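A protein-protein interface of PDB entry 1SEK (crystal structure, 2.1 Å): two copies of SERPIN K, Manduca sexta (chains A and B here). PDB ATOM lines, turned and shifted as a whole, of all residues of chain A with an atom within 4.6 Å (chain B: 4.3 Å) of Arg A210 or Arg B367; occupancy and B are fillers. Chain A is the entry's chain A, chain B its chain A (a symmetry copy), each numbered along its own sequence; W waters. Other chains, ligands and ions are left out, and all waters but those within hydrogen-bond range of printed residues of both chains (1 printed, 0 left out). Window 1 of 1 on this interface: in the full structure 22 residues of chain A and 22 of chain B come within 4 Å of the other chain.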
ATOM      1  N   VAL A 209      15.783  20.246 -21.155  1.00  0.00           N
ATOM      2  CA  VAL A 209      17.087  19.751 -20.750  1.00  0.00           C
ATOM      3  C   VAL A 209      18.092  20.096 -21.841  1.00  0.00           C
ATOM      4  O   VAL A 209      17.733  20.672 -22.879  1.00  0.00           O
ATOM      5  CB  VAL A 209      17.077  18.216 -20.630  1.00  0.00           C
ATOM      6  CG1 VAL A 209      16.082  17.705 -19.588  1.00  0.00           C
ATOM      7  CG2 VAL A 209      16.704  17.518 -21.939  1.00  0.00           C
ATOM      8  N   ARG A 210      19.313  19.738 -21.559  1.00  0.00           N
ATOM      9  CA  ARG A 210      20.413  19.840 -22.513  1.00  0.00           C
ATOM     10  C   ARG A 210      20.703  18.406 -22.921  1.00  0.00           C
ATOM     11  O   ARG A 210      20.990  17.552 -22.076  1.00  0.00           O
ATOM     12  CB  ARG A 210      21.616  20.508 -21.852  1.00  0.00           C
ATOM     13  CG  ARG A 210      21.260  21.821 -21.154  1.00  0.00           C
ATOM     14  CD  ARG A 210      21.962  23.032 -21.769  1.00  0.00           C
ATOM     15  NE  ARG A 210      23.402  23.059 -21.484  1.00  0.00           N
ATOM     16  CZ  ARG A 210      24.273  23.865 -22.101  1.00  0.00           C
ATOM     17  NH1 ARG A 210      23.868  24.724 -23.046  1.00  0.00           N
ATOM     18  NH2 ARG A 210      25.586  23.886 -21.838  1.00  0.00           N
ATOM     19  N   TYR A 211      20.606  18.138 -24.197  1.00  0.00           N
ATOM     20  CA  TYR A 211      20.746  16.764 -24.689  1.00  0.00           C
ATOM     21  C   TYR A 211      21.788  16.674 -25.796  1.00  0.00           C
ATOM     22  O   TYR A 211      22.111  17.668 -26.458  1.00  0.00           O
ATOM     23  CB  TYR A 211      19.385  16.316 -25.210  1.00  0.00           C
ATOM     24  CG  TYR A 211      19.376  14.929 -25.840  1.00  0.00           C
ATOM     25  CD1 TYR A 211      19.747  14.774 -27.178  1.00  0.00           C
ATOM     26  CD2 TYR A 211      18.986  13.821 -25.081  1.00  0.00           C
ATOM     27  CE1 TYR A 211      19.712  13.505 -27.766  1.00  0.00           C
ATOM     28  CE2 TYR A 211      18.954  12.553 -25.667  1.00  0.00           C
ATOM     29  CZ  TYR A 211      19.314  12.395 -27.011  1.00  0.00           C
ATOM     30  OH  TYR A 211      19.274  11.164 -27.584  1.00  0.00           O
ATOM     31  N   ALA A 212      22.284  15.464 -25.968  1.00  0.00           N
ATOM     32  CA  ALA A 212      23.288  15.186 -26.989  1.00  0.00           C
ATOM     33  C   ALA A 212      23.552  13.692 -27.122  1.00  0.00           C
ATOM     34  O   ALA A 212      23.648  12.962 -26.127  1.00  0.00           O
ATOM     35  CB  ALA A 212      24.613  15.860 -26.622  1.00  0.00           C
ATOM     36  N   MET A 221      23.723  11.749 -23.643  1.00  0.00           N
ATOM     37  CA  MET A 221      23.985  12.586 -22.488  1.00  0.00           C
ATOM     38  C   MET A 221      22.803  13.505 -22.254  1.00  0.00           C
ATOM     39  O   MET A 221      22.216  14.039 -23.193  1.00  0.00           O
ATOM     40  CB  MET A 221      25.262  13.407 -22.700  1.00  0.00           C
ATOM     41  CG  MET A 221      25.691  14.228 -21.483  1.00  0.00           C
ATOM     42  SD  MET A 221      27.157  15.233 -21.831  1.00  0.00           S
ATOM     43  CE  MET A 221      28.208  14.744 -20.492  1.00  0.00           C
ATOM     44  N   ILE A 222      22.447  13.661 -20.989  1.00  0.00           N
ATOM     45  CA  ILE A 222      21.351  14.521 -20.606  1.00  0.00           C
ATOM     46  C   ILE A 222      21.806  15.363 -19.419  1.00  0.00           C
ATOM     47  O   ILE A 222      22.539  14.892 -18.548  1.00  0.00           O
ATOM     48  CB  ILE A 222      20.113  13.701 -20.200  1.00  0.00           C
ATOM     49  CG1 ILE A 222      19.686  12.786 -21.352  1.00  0.00           C
ATOM     50  CG2 ILE A 222      18.973  14.630 -19.842  1.00  0.00           C
ATOM     51  CD1 ILE A 222      19.812  11.299 -21.056  1.00  0.00           C
ATOM     52  N   GLU A 223      21.381  16.620 -19.401  1.00  0.00           N
ATOM     53  CA  GLU A 223      21.723  17.524 -18.318  1.00  0.00           C
ATOM     54  C   GLU A 223      20.461  18.221 -17.828  1.00  0.00           C
ATOM     55  O   GLU A 223      19.793  18.928 -18.585  1.00  0.00           O
ATOM     56  CB  GLU A 223      22.751  18.550 -18.789  1.00  0.00           C
ATOM     57  CG  GLU A 223      23.377  19.331 -17.660  1.00  0.00           C
ATOM     58  CD  GLU A 223      24.374  20.345 -18.152  1.00  0.00           C
ATOM     59  OE1 GLU A 223      25.429  19.930 -18.676  1.00  0.00           O
ATOM     60  OE2 GLU A 223      24.097  21.554 -18.018  1.00  0.00           O
ATOM     61  N   GLU A 261      30.231  17.371 -23.709  1.00  0.00           N
ATOM     62  CA  GLU A 261      29.473  18.568 -23.370  1.00  0.00           C
ATOM     63  C   GLU A 261      29.444  19.602 -24.497  1.00  0.00           C
ATOM     64  O   GLU A 261      28.525  20.419 -24.581  1.00  0.00           O
ATOM     65  CB  GLU A 261      30.052  19.194 -22.104  1.00  0.00           C
ATOM     66  CG  GLU A 261      29.588  18.514 -20.832  1.00  0.00           C
ATOM     67  CD  GLU A 261      30.398  18.929 -19.623  1.00  0.00           C
ATOM     68  OE1 GLU A 261      31.642  18.934 -19.711  1.00  0.00           O
ATOM     69  OE2 GLU A 261      29.787  19.252 -18.584  1.00  0.00           O
ATOM     70  N   GLU A 262      30.453  19.569 -25.359  1.00  0.00           N
ATOM     71  CA  GLU A 262      30.515  20.489 -26.484  1.00  0.00           C
ATOM     72  C   GLU A 262      29.399  20.149 -27.470  1.00  0.00           C
ATOM     73  O   GLU A 262      29.060  20.951 -28.335  1.00  0.00           O
ATOM     74  CB  GLU A 262      31.872  20.381 -27.185  1.00  0.00           C
ATOM     75  CG  GLU A 262      32.932  21.343 -26.656  1.00  0.00           C
ATOM     76  CD  GLU A 262      32.588  22.801 -26.912  1.00  0.00           C
ATOM     77  OE1 GLU A 262      32.688  23.241 -28.080  1.00  0.00           O
ATOM     78  OE2 GLU A 262      32.218  23.507 -25.948  1.00  0.00           O
ATOM     79  N   ARG A 263      28.824  18.958 -27.325  1.00  0.00           N
ATOM     80  CA  ARG A 263      27.756  18.510 -28.212  1.00  0.00           C
ATOM     81  C   ARG A 263      26.365  18.870 -27.706  1.00  0.00           C
ATOM     82  O   ARG A 263      25.394  18.829 -28.460  1.00  0.00           O
ATOM     83  CB  ARG A 263      27.840  16.993 -28.412  1.00  0.00           C
ATOM     84  CG  ARG A 263      28.936  16.546 -29.374  1.00  0.00           C
ATOM     85  CD  ARG A 263      29.013  15.029 -29.465  1.00  0.00           C
ATOM     86  NE  ARG A 263      27.923  14.492 -30.269  1.00  0.00           N
ATOM     87  CZ  ARG A 263      27.873  14.554 -31.599  1.00  0.00           C
ATOM     88  NH1 ARG A 263      28.860  15.125 -32.271  1.00  0.00           N
ATOM     89  NH2 ARG A 263      26.840  14.039 -32.258  1.00  0.00           N
ATOM     90  N   LEU A 264      26.272  19.243 -26.434  1.00  0.00           N
ATOM     91  CA  LEU A 264      24.989  19.575 -25.824  1.00  0.00           C
ATOM     92  C   LEU A 264      24.224  20.713 -26.500  1.00  0.00           C
ATOM     93  O   LEU A 264      24.815  21.698 -26.923  1.00  0.00           O
ATOM     94  CB  LEU A 264      25.194  19.919 -24.341  1.00  0.00           C
ATOM     95  CG  LEU A 264      24.801  18.879 -23.276  1.00  0.00           C
ATOM     96  CD1 LEU A 264      25.081  17.472 -23.759  1.00  0.00           C
ATOM     97  CD2 LEU A 264      25.585  19.152 -21.991  1.00  0.00           C
ATOM     98  N   TYR A 265      22.906  20.560 -26.598  1.00  0.00           N
ATOM     99  CA  TYR A 265      22.036  21.589 -27.168  1.00  0.00           C
ATOM    100  C   TYR A 265      20.716  21.538 -26.397  1.00  0.00           C
ATOM    101  O   TYR A 265      20.360  20.497 -25.846  1.00  0.00           O
ATOM    102  CB  TYR A 265      21.818  21.370 -28.679  1.00  0.00           C
ATOM    103  CG  TYR A 265      20.969  20.172 -29.043  1.00  0.00           C
ATOM    104  CD1 TYR A 265      19.577  20.260 -29.066  1.00  0.00           C
ATOM    105  CD2 TYR A 265      21.557  18.946 -29.352  1.00  0.00           C
ATOM    106  CE1 TYR A 265      18.792  19.152 -29.385  1.00  0.00           C
ATOM    107  CE2 TYR A 265      20.783  17.838 -29.670  1.00  0.00           C
ATOM    108  CZ  TYR A 265      19.403  17.946 -29.681  1.00  0.00           C
ATOM    109  OH  TYR A 265      18.630  16.839 -29.957  1.00  0.00           O
ATOM    110  N   ASN A 266      20.003  22.658 -26.340  1.00  0.00           N
ATOM    111  CA  ASN A 266      18.747  22.729 -25.604  1.00  0.00           C
ATOM    112  C   ASN A 266      17.556  22.151 -26.342  1.00  0.00           C
ATOM    113  O   ASN A 266      17.399  22.344 -27.541  1.00  0.00           O
ATOM    114  CB  ASN A 266      18.451  24.173 -25.233  1.00  0.00           C
ATOM    115  CG  ASN A 266      19.476  24.740 -24.278  1.00  0.00           C
ATOM    116  OD1 ASN A 266      19.180  24.967 -23.107  1.00  0.00           O
ATOM    117  ND2 ASN A 266      20.690  24.970 -24.770  1.00  0.00           N
ATOM    118  N   ARG B  12      25.667  25.597 -35.535  1.00  0.00           N
ATOM    119  CA  ARG B  12      26.508  26.352 -34.622  1.00  0.00           C
ATOM    120  C   ARG B  12      27.799  26.781 -35.293  1.00  0.00           C
ATOM    121  O   ARG B  12      28.184  27.952 -35.232  1.00  0.00           O
ATOM    122  CB  ARG B  12      26.835  25.509 -33.392  1.00  0.00           C
ATOM    123  CG  ARG B  12      26.889  26.306 -32.109  1.00  0.00           C
ATOM    124  CD  ARG B  12      26.600  25.436 -30.895  1.00  0.00           C
ATOM    125  NE  ARG B  12      27.216  24.121 -31.017  1.00  0.00           N
ATOM    126  CZ  ARG B  12      26.586  22.976 -30.771  1.00  0.00           C
ATOM    127  NH1 ARG B  12      25.317  22.986 -30.389  1.00  0.00           N
ATOM    128  NH2 ARG B  12      27.225  21.819 -30.910  1.00  0.00           N
ATOM    129  N   LYS B 364      23.491  35.674 -26.675  1.00  0.00           N
ATOM    130  CA  LYS B 364      23.687  34.239 -26.825  1.00  0.00           C
ATOM    131  C   LYS B 364      22.413  33.479 -26.471  1.00  0.00           C
ATOM    132  O   LYS B 364      21.886  33.623 -25.367  1.00  0.00           O
ATOM    133  CB  LYS B 364      24.820  33.774 -25.903  1.00  0.00           C
ATOM    134  CG  LYS B 364      25.860  32.898 -26.569  1.00  0.00           C
ATOM    135  CD  LYS B 364      26.757  33.711 -27.488  1.00  0.00           C
ATOM    136  CE  LYS B 364      27.633  32.814 -28.348  1.00  0.00           C
ATOM    137  NZ  LYS B 364      28.200  31.672 -27.576  1.00  0.00           N
ATOM    138  N   TYR B 365      21.920  32.685 -27.418  1.00  0.00           N
ATOM    139  CA  TYR B 365      20.729  31.866 -27.208  1.00  0.00           C
ATOM    140  C   TYR B 365      21.060  30.462 -27.697  1.00  0.00           C
ATOM    141  O   TYR B 365      21.621  30.301 -28.779  1.00  0.00           O
ATOM    142  CB  TYR B 365      19.537  32.407 -27.997  1.00  0.00           C
ATOM    143  CG  TYR B 365      18.306  31.536 -27.882  1.00  0.00           C
ATOM    144  CD1 TYR B 365      17.431  31.676 -26.806  1.00  0.00           C
ATOM    145  CD2 TYR B 365      18.019  30.560 -28.840  1.00  0.00           C
ATOM    146  CE1 TYR B 365      16.302  30.866 -26.685  1.00  0.00           C
ATOM    147  CE2 TYR B 365      16.891  29.746 -28.727  1.00  0.00           C
ATOM    148  CZ  TYR B 365      16.039  29.907 -27.646  1.00  0.00           C
ATOM    149  OH  TYR B 365      14.920  29.116 -27.521  1.00  0.00           O
ATOM    150  N   ASN B 366      20.736  29.449 -26.899  1.00  0.00           N
ATOM    151  CA  ASN B 366      21.020  28.066 -27.274  1.00  0.00           C
ATOM    152  C   ASN B 366      22.435  27.931 -27.825  1.00  0.00           C
ATOM    153  O   ASN B 366      22.659  27.254 -28.832  1.00  0.00           O
ATOM    154  CB  ASN B 366      20.015  27.585 -28.328  1.00  0.00           C
ATOM    155  CG  ASN B 366      20.236  26.126 -28.734  1.00  0.00           C
ATOM    156  OD1 ASN B 366      20.634  25.286 -27.915  1.00  0.00           O
ATOM    157  ND2 ASN B 366      19.978  25.822 -30.010  1.00  0.00           N
ATOM    158  N   ARG B 367      23.385  28.594 -27.173  1.00  0.00           N
ATOM    159  CA  ARG B 367      24.786  28.542 -27.588  1.00  0.00           C
ATOM    160  C   ARG B 367      25.082  29.189 -28.949  1.00  0.00           C
ATOM    161  O   ARG B 367      26.161  28.987 -29.504  1.00  0.00           O
ATOM    162  CB  ARG B 367      25.275  27.088 -27.585  1.00  0.00           C
ATOM    163  CG  ARG B 367      25.437  26.491 -26.185  1.00  0.00           C
ATOM    164  CD  ARG B 367      25.971  25.061 -26.218  1.00  0.00           C
ATOM    165  NE  ARG B 367      27.317  24.993 -26.782  1.00  0.00           N
ATOM    166  CZ  ARG B 367      27.873  23.890 -27.278  1.00  0.00           C
ATOM    167  NH1 ARG B 367      27.199  22.747 -27.277  1.00  0.00           N
ATOM    168  NH2 ARG B 367      29.099  23.930 -27.786  1.00  0.00           N
ATOM    169  N   ASN B 368      24.133  29.956 -29.484  1.00  0.00           N
ATOM    170  CA  ASN B 368      24.327  30.646 -30.766  1.00  0.00           C
ATOM    171  C   ASN B 368      24.199  32.165 -30.575  1.00  0.00           C
ATOM    172  O   ASN B 368      23.291  32.634 -29.890  1.00  0.00           O
ATOM    173  CB  ASN B 368      23.276  30.205 -31.788  1.00  0.00           C
ATOM    174  CG  ASN B 368      23.597  28.870 -32.428  1.00  0.00           C
ATOM    175  OD1 ASN B 368      24.693  28.659 -32.941  1.00  0.00           O
ATOM    176  ND2 ASN B 368      22.634  27.964 -32.405  1.00  0.00           N
HETATM  177  O   HOH W   1      25.112  19.513 -31.317  1.00  0.00           O
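The backbone carbonyl oxygen of Glu A262 sits at hydrogen-bond distance from the guanidinium group of Arg B12 (3.3 Å). The side-chain carboxylate (OE2) of Glu A262 is in salt-bridge range of the guanidinium group (NH2) of Arg B367 (3.6 Å). The backbone carbonyl oxygen of Leu A264 is in hydrogen-bond range of the guanidinium group of Arg B367, at 2.6 Å. The side-chain amide oxygen (OD1) of Asn B366 lies within hydrogen-bond range of the backbone NH (N) of Asn A266 (3.1 Å).
The guanidinium group of Arg A210 is in salt-bridge range of the side-chain carboxylate of Glu A223, 3.8 Å away.
NH1 of Arg A210 touches CD of Arg B367, 3.8 Å away. Arg B367 touches Glu A261 (NH1 to O, 3.8 Å). Arg A263 touches Arg B367 (C to NH1, 3.99 Å). Leu A264 touches Arg B12.
Of chain B, only Arg B367 (3.8 Å) comes within 4 Å of Arg A210. Of the printed residues of chain A, Arg B367 touches Arg A210, Glu A261, Glu A262, Arg A263 and Leu A264. Of the printed residues of chain B, Leu A264 touches Arg B12 (3.7 Å) and Arg B367 (2.6 Å). Of the printed residues of chain B, Asn A266 touches Asn B366 (3.1 Å). Printed residues of chain B within 4 Å of Glu A262: Arg B12 and Arg B367. Of the printed residues of chain A, Asn B366 touches Asn A266. Printed residues of chain B within 4 Å of Glu A261: Arg B367 (3.8 Å). Tyr A265 touches none of the printed residues of chain B. Ile A222 touches none of the printed residues of chain B. The nearest printed residue of chain B that does not touch Arg A210 is Asn B366 (5.9 Å). The nearest printed residue of chain A that does not touch Arg B367 is Tyr A265 (4.9 Å). The nearest printed residue of chain B that does not touch Glu A261 is Arg B12 (6.6 Å).
Printed residues of chain A that touch a printed residue of chain B: Arg A210, Glu A261, Glu A262, Arg A263, Leu A264 and Asn A266. Printed residues of chain B that touch a printed residue of chain A: Arg B12, Asn B366 and Arg B367.
No position is printed for both chains. Of the 8 pairs that touch across the chains among the printed residues, none has its exchanged pair printed and touching as well.
Water W1 lies within hydrogen-bond range of the backbone carbonyl oxygen of Arg A263 (3.0 Å) and the guanidinium group of Arg B12 (3.2 Å).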
